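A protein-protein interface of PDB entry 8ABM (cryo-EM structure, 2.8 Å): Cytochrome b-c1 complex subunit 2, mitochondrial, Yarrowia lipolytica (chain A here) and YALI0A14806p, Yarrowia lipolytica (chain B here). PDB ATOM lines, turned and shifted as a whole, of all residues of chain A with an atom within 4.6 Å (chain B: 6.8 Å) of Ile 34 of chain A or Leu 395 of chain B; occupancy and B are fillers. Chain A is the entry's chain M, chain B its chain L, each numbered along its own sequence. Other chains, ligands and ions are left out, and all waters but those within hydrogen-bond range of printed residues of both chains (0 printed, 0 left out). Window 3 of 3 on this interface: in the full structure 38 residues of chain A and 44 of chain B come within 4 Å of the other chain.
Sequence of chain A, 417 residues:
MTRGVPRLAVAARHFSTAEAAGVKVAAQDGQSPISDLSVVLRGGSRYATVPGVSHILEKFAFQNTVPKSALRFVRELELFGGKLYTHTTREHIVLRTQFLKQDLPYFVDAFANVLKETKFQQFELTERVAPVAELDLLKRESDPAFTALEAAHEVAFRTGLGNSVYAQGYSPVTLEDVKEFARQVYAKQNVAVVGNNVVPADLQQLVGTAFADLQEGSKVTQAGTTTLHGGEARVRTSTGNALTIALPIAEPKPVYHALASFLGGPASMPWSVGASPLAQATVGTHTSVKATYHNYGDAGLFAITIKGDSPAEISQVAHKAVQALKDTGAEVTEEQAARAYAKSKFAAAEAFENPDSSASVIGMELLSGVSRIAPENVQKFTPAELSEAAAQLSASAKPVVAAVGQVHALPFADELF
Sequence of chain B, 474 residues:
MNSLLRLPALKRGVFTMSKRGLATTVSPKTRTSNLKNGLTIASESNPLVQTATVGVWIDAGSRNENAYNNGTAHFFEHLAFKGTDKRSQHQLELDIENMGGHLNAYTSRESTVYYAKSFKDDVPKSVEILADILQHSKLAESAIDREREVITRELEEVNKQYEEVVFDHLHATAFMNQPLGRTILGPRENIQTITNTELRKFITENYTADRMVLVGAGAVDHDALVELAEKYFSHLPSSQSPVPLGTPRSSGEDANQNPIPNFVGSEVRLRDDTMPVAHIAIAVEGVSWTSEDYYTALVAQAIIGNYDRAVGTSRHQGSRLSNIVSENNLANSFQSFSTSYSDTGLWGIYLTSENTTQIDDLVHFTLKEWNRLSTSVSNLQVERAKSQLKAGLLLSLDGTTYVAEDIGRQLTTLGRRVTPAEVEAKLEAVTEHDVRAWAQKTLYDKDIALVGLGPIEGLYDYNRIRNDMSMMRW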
ATOM      1  N   SER A  32       8.643  31.526   8.560  1.00  0.00           N
ATOM      2  CA  SER A  32       8.182  30.599   7.546  1.00  0.00           C
ATOM      3  C   SER A  32       9.247  29.523   7.424  1.00  0.00           C
ATOM      4  O   SER A  32      10.399  29.777   7.766  1.00  0.00           O
ATOM      5  CB  SER A  32       7.918  31.302   6.223  1.00  0.00           C
ATOM      6  OG  SER A  32       8.881  30.977   5.243  1.00  0.00           O
ATOM      7  N   PRO A  33       8.926  28.314   6.919  1.00  0.00           N
ATOM      8  CA  PRO A  33       9.947  27.284   6.780  1.00  0.00           C
ATOM      9  C   PRO A  33      10.793  27.404   5.514  1.00  0.00           C
ATOM     10  O   PRO A  33      11.771  26.671   5.377  1.00  0.00           O
ATOM     11  CB  PRO A  33       9.128  25.989   6.804  1.00  0.00           C
ATOM     12  CG  PRO A  33       7.805  26.379   6.175  1.00  0.00           C
ATOM     13  CD  PRO A  33       7.594  27.845   6.502  1.00  0.00           C
ATOM     14  N   ILE A  34      10.456  28.362   4.629  1.00  0.00           N
ATOM     15  CA  ILE A  34      11.096  28.441   3.322  1.00  0.00           C
ATOM     16  C   ILE A  34      11.877  29.742   3.172  1.00  0.00           C
ATOM     17  O   ILE A  34      11.363  30.840   3.371  1.00  0.00           O
ATOM     18  CB  ILE A  34      10.133  28.179   2.141  1.00  0.00           C
ATOM     19  CG1 ILE A  34       8.863  29.030   2.216  1.00  0.00           C
ATOM     20  CG2 ILE A  34       9.826  26.691   2.045  1.00  0.00           C
ATOM     21  CD1 ILE A  34       8.216  29.323   0.873  1.00  0.00           C
ATOM     22  N   SER A  35      13.139  29.589   2.769  1.00  0.00           N
ATOM     23  CA  SER A  35      14.025  30.716   2.542  1.00  0.00           C
ATOM     24  C   SER A  35      14.275  30.883   1.046  1.00  0.00           C
ATOM     25  O   SER A  35      14.296  29.901   0.303  1.00  0.00           O
ATOM     26  CB  SER A  35      15.305  30.492   3.271  1.00  0.00           C
ATOM     27  OG  SER A  35      15.078  30.442   4.675  1.00  0.00           O
ATOM     28  N   ASP A  36      14.449  32.141   0.622  1.00  0.00           N
ATOM     29  CA  ASP A  36      14.893  32.457  -0.722  1.00  0.00           C
ATOM     30  C   ASP A  36      16.246  33.156  -0.663  1.00  0.00           C
ATOM     31  O   ASP A  36      16.345  34.303  -0.237  1.00  0.00           O
ATOM     32  CB  ASP A  36      13.862  33.321  -1.459  1.00  0.00           C
ATOM     33  CG  ASP A  36      12.562  32.603  -1.820  1.00  0.00           C
ATOM     34  OD1 ASP A  36      12.535  31.348  -1.785  1.00  0.00           O
ATOM     35  OD2 ASP A  36      11.574  33.309  -2.163  1.00  0.00           O
ATOM     36  N   GLY A  81      15.019  19.183  -1.656  1.00  0.00           N
ATOM     37  CA  GLY A  81      13.804  19.643  -2.302  1.00  0.00           C
ATOM     38  C   GLY A  81      13.827  21.133  -2.641  1.00  0.00           C
ATOM     39  O   GLY A  81      12.768  21.732  -2.808  1.00  0.00           O
ATOM     40  N   LYS A  83      14.576  24.508  -5.092  1.00  0.00           N
ATOM     41  CA  LYS A  83      14.312  24.845  -6.475  1.00  0.00           C
ATOM     42  C   LYS A  83      15.247  25.963  -6.879  1.00  0.00           C
ATOM     43  O   LYS A  83      15.687  26.753  -6.046  1.00  0.00           O
ATOM     44  CB  LYS A  83      12.919  25.446  -6.645  1.00  0.00           C
ATOM     45  CG  LYS A  83      11.752  24.612  -6.149  1.00  0.00           C
ATOM     46  CD  LYS A  83      11.333  23.444  -7.044  1.00  0.00           C
ATOM     47  CE  LYS A  83       9.834  23.303  -7.243  1.00  0.00           C
ATOM     48  NZ  LYS A  83       9.051  23.947  -6.158  1.00  0.00           N
ATOM     49  N   GLN A  98      15.280  28.494  -3.718  1.00  0.00           N
ATOM     50  CA  GLN A  98      14.260  28.412  -2.700  1.00  0.00           C
ATOM     51  C   GLN A  98      14.462  27.085  -1.986  1.00  0.00           C
ATOM     52  O   GLN A  98      14.517  26.052  -2.643  1.00  0.00           O
ATOM     53  CB  GLN A  98      12.942  28.439  -3.451  1.00  0.00           C
ATOM     54  CG  GLN A  98      11.727  28.681  -2.586  1.00  0.00           C
ATOM     55  CD  GLN A  98      10.594  29.107  -3.487  1.00  0.00           C
ATOM     56  OE1 GLN A  98      10.024  28.306  -4.228  1.00  0.00           O
ATOM     57  NE2 GLN A  98      10.267  30.389  -3.433  1.00  0.00           N
ATOM     58  N   PHE A  99      14.581  27.109  -0.657  1.00  0.00           N
ATOM     59  CA  PHE A  99      14.868  25.881   0.072  1.00  0.00           C
ATOM     60  C   PHE A  99      14.311  25.981   1.487  1.00  0.00           C
ATOM     61  O   PHE A  99      13.761  27.002   1.869  1.00  0.00           O
ATOM     62  CB  PHE A  99      16.379  25.626   0.085  1.00  0.00           C
ATOM     63  CG  PHE A  99      17.160  26.855   0.454  1.00  0.00           C
ATOM     64  CD1 PHE A  99      17.513  27.769  -0.529  1.00  0.00           C
ATOM     65  CD2 PHE A  99      17.495  27.129   1.777  1.00  0.00           C
ATOM     66  CE1 PHE A  99      18.186  28.932  -0.186  1.00  0.00           C
ATOM     67  CE2 PHE A  99      18.167  28.297   2.117  1.00  0.00           C
ATOM     68  CZ  PHE A  99      18.507  29.199   1.131  1.00  0.00           C
ATOM     69  N   LEU A 100      14.480  24.921   2.281  1.00  0.00           N
ATOM     70  CA  LEU A 100      14.072  24.981   3.676  1.00  0.00           C
ATOM     71  C   LEU A 100      15.112  25.755   4.471  1.00  0.00           C
ATOM     72  O   LEU A 100      16.290  25.681   4.149  1.00  0.00           O
ATOM     73  CB  LEU A 100      13.943  23.559   4.212  1.00  0.00           C
ATOM     74  CG  LEU A 100      12.856  22.740   3.532  1.00  0.00           C
ATOM     75  CD1 LEU A 100      12.953  21.279   3.926  1.00  0.00           C
ATOM     76  CD2 LEU A 100      11.471  23.312   3.823  1.00  0.00           C
ATOM     77  N   ASN A 196      15.737  36.349   1.725  1.00  0.00           N
ATOM     78  CA  ASN A 196      14.374  36.421   2.221  1.00  0.00           C
ATOM     79  C   ASN A 196      14.085  35.260   3.172  1.00  0.00           C
ATOM     80  O   ASN A 196      14.129  34.100   2.762  1.00  0.00           O
ATOM     81  CB  ASN A 196      13.383  36.368   1.063  1.00  0.00           C
ATOM     82  CG  ASN A 196      12.190  37.255   1.325  1.00  0.00           C
ATOM     83  OD1 ASN A 196      11.541  37.146   2.366  1.00  0.00           O
ATOM     84  ND2 ASN A 196      11.921  38.164   0.398  1.00  0.00           N
ATOM     85  N   ASN A 197      13.725  35.592   4.420  1.00  0.00           N
ATOM     86  CA  ASN A 197      13.437  34.634   5.489  1.00  0.00           C
ATOM     87  C   ASN A 197      14.724  33.896   5.862  1.00  0.00           C
ATOM     88  O   ASN A 197      14.749  32.690   6.090  1.00  0.00           O
ATOM     89  CB  ASN A 197      12.175  33.787   5.240  1.00  0.00           C
ATOM     90  CG  ASN A 197      11.878  32.756   6.314  1.00  0.00           C
ATOM     91  OD1 ASN A 197      11.565  33.080   7.457  1.00  0.00           O
ATOM     92  ND2 ASN A 197      11.933  31.491   5.939  1.00  0.00           N
ATOM     93  N   LEU B 389       9.382  16.036  -1.119  1.00  0.00           N
ATOM     94  CA  LEU B 389       7.992  16.417  -0.893  1.00  0.00           C
ATOM     95  C   LEU B 389       7.860  17.212   0.402  1.00  0.00           C
ATOM     96  O   LEU B 389       7.008  18.096   0.527  1.00  0.00           O
ATOM     97  CB  LEU B 389       7.147  15.149  -0.787  1.00  0.00           C
ATOM     98  CG  LEU B 389       6.363  14.731  -2.025  1.00  0.00           C
ATOM     99  CD1 LEU B 389       5.548  13.494  -1.697  1.00  0.00           C
ATOM    100  CD2 LEU B 389       5.436  15.840  -2.507  1.00  0.00           C
ATOM    101  N   LYS B 390       8.683  16.826   1.380  1.00  0.00           N
ATOM    102  CA  LYS B 390       8.718  17.452   2.685  1.00  0.00           C
ATOM    103  C   LYS B 390       8.949  18.950   2.494  1.00  0.00           C
ATOM    104  O   LYS B 390       8.338  19.749   3.193  1.00  0.00           O
ATOM    105  CB  LYS B 390       9.644  16.651   3.612  1.00  0.00           C
ATOM    106  CG  LYS B 390      10.671  17.428   4.421  1.00  0.00           C
ATOM    107  CD  LYS B 390      10.079  18.027   5.681  1.00  0.00           C
ATOM    108  CE  LYS B 390      11.000  18.984   6.408  1.00  0.00           C
ATOM    109  NZ  LYS B 390      10.444  19.392   7.722  1.00  0.00           N
ATOM    110  N   ALA B 391       9.759  19.307   1.488  1.00  0.00           N
ATOM    111  CA  ALA B 391       9.962  20.697   1.116  1.00  0.00           C
ATOM    112  C   ALA B 391       8.840  21.184   0.201  1.00  0.00           C
ATOM    113  O   ALA B 391       8.320  22.276   0.406  1.00  0.00           O
ATOM    114  CB  ALA B 391      11.314  20.871   0.478  1.00  0.00           C
ATOM    115  N   GLY B 392       8.488  20.377  -0.805  1.00  0.00           N
ATOM    116  CA  GLY B 392       7.598  20.789  -1.881  1.00  0.00           C
ATOM    117  C   GLY B 392       6.229  21.257  -1.389  1.00  0.00           C
ATOM    118  O   GLY B 392       5.647  22.170  -1.965  1.00  0.00           O
ATOM    119  N   LEU B 393       5.731  20.627  -0.318  1.00  0.00           N
ATOM    120  CA  LEU B 393       4.413  20.928   0.223  1.00  0.00           C
ATOM    121  C   LEU B 393       4.425  22.242   0.991  1.00  0.00           C
ATOM    122  O   LEU B 393       3.369  22.812   1.243  1.00  0.00           O
ATOM    123  CB  LEU B 393       3.950  19.766   1.105  1.00  0.00           C
ATOM    124  CG  LEU B 393       3.623  18.486   0.340  1.00  0.00           C
ATOM    125  CD1 LEU B 393       3.499  17.308   1.285  1.00  0.00           C
ATOM    126  CD2 LEU B 393       2.361  18.640  -0.500  1.00  0.00           C
ATOM    127  N   LEU B 394       5.620  22.706   1.362  1.00  0.00           N
ATOM    128  CA  LEU B 394       5.773  23.986   2.033  1.00  0.00           C
ATOM    129  C   LEU B 394       6.189  25.080   1.050  1.00  0.00           C
ATOM    130  O   LEU B 394       5.828  26.238   1.265  1.00  0.00           O
ATOM    131  CB  LEU B 394       6.777  23.842   3.183  1.00  0.00           C
ATOM    132  CG  LEU B 394       6.497  22.696   4.152  1.00  0.00           C
ATOM    133  CD1 LEU B 394       7.650  22.508   5.119  1.00  0.00           C
ATOM    134  CD2 LEU B 394       5.198  22.920   4.908  1.00  0.00           C
ATOM    135  N   LEU B 395       6.953  24.713  -0.003  1.00  0.00           N
ATOM    136  CA  LEU B 395       7.540  25.646  -0.962  1.00  0.00           C
ATOM    137  C   LEU B 395       6.464  26.293  -1.834  1.00  0.00           C
ATOM    138  O   LEU B 395       6.622  27.434  -2.271  1.00  0.00           O
ATOM    139  CB  LEU B 395       8.581  24.927  -1.836  1.00  0.00           C
ATOM    140  CG  LEU B 395      10.044  25.299  -1.586  1.00  0.00           C
ATOM    141  CD1 LEU B 395      10.613  24.581  -0.376  1.00  0.00           C
ATOM    142  CD2 LEU B 395      10.890  24.992  -2.807  1.00  0.00           C
ATOM    143  N   SER B 396       5.419  25.521  -2.149  1.00  0.00           N
ATOM    144  CA  SER B 396       4.263  25.992  -2.900  1.00  0.00           C
ATOM    145  C   SER B 396       3.691  27.285  -2.314  1.00  0.00           C
ATOM    146  O   SER B 396       3.243  28.146  -3.070  1.00  0.00           O
ATOM    147  CB  SER B 396       3.221  24.908  -3.035  1.00  0.00           C
ATOM    148  OG  SER B 396       3.176  24.094  -1.874  1.00  0.00           O
ATOM    149  N   LEU B 397       3.717  27.418  -0.978  1.00  0.00           N
ATOM    150  CA  LEU B 397       3.127  28.549  -0.264  1.00  0.00           C
ATOM    151  C   LEU B 397       4.104  29.722  -0.179  1.00  0.00           C
ATOM    152  O   LEU B 397       4.797  29.922   0.819  1.00  0.00           O
ATOM    153  CB  LEU B 397       2.703  28.099   1.138  1.00  0.00           C
ATOM    154  CG  LEU B 397       2.426  26.611   1.322  1.00  0.00           C
ATOM    155  CD1 LEU B 397       2.365  26.267   2.799  1.00  0.00           C
ATOM    156  CD2 LEU B 397       1.123  26.199   0.644  1.00  0.00           C
ATOM    157  N   ASP B 398       4.117  30.531  -1.249  1.00  0.00           N
ATOM    158  CA  ASP B 398       4.993  31.676  -1.436  1.00  0.00           C
ATOM    159  C   ASP B 398       4.317  32.976  -0.974  1.00  0.00           C
ATOM    160  O   ASP B 398       4.617  33.492   0.107  1.00  0.00           O
ATOM    161  CB  ASP B 398       5.382  31.790  -2.915  1.00  0.00           C
ATOM    162  CG  ASP B 398       6.114  30.579  -3.473  1.00  0.00           C
ATOM    163  OD1 ASP B 398       7.254  30.315  -3.032  1.00  0.00           O
ATOM    164  OD2 ASP B 398       5.530  29.890  -4.329  1.00  0.00           O
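OD1 of Asp 36 of chain A sits close to NE2 of Gln 98 of chain A (3.0 Å). The backbone NH of Lys 83 of chain A is in hydrogen-bond range of the backbone carbonyl oxygen of Gln 98 of chain A, 2.9 Å away. The backbone carbonyl oxygen (O) of Ile 34 of chain A is in hydrogen-bond range of the side-chain amide nitrogen (ND2) of Asn 197 of chain A (2.7 Å). The side-chain hydroxyl of Ser 32 of chain A lies within hydrogen-bond range of the backbone carbonyl oxygen of Ile 34 of chain A (3.1 Å).
Ile 34 of chain A touches Leu 394 of chain B (CD1 to O, 3.9 Å). CG2 of Ile 34 of chain A touches CD1 of Leu 395 of chain B (3.3 Å). Leu 397 of chain B touches Ile 34 of chain A (O to CD1, 3.5 Å). CB of Ala 391 of chain B touches O of Gly 81 of chain A, at 3.7 Å. CD2 of Leu 395 of chain B touches O of Gly 81 of chain A (3.8 Å). Lys 83 of chain A touches Leu 395 of chain B (CG to CD2, 3.5 Å). Gln 98 of chain A touches Leu 395 of chain B (OE1 to CD2, 3.7 Å). Leu 100 of chain A touches Lys 390 of chain B (CD1 to CE, 3.9 Å). Ala 391 of chain B touches Leu 100 of chain A (CB to CD1, 3.8 Å).
Ile 34 of chain A touches just these residues of chain B: Leu 394, Leu 395 and Leu 397. Of the printed residues of chain B, Lys 83 of chain A touches Leu 395. Of the printed residues of chain A, Leu 397 of chain B touches Ile 34. Of the printed residues of chain A, Asp 398 of chain B touches Gln 98. Printed residues of chain B within 4 Å of Gly 81 of chain A: Ala 391 and Leu 395. Leu 393 of chain B touches none of the printed residues of chain A. Gly 392 of chain B touches none of the printed residues of chain A. The nearest residue of chain B that does not touch Ile 34 of chain A is Asp 398 of chain B (4.1 Å). The nearest residue of chain A that does not touch Leu 395 of chain B is Phe 99 of chain A (4.4 Å).
The side-chain amide nitrogen of Gln 98 of chain A sits at hydrogen-bond distance from the side-chain carboxylate of Asp 398 of chain B.
Of the 10 printed residues of chain B, 6 touch a printed residue of chain A. Printed residues of chain B that touch a printed residue of chain A: Lys 390, Ala 391, Leu 394, Leu 395, Leu 397 and Asp 398. Hydrophobic or aromatic side chains of chain B within 4 Å of the printed part of chain A: Ala 391 and Leu 395. Of the 12 printed residues of chain A, 5 touch a printed residue of chain B.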
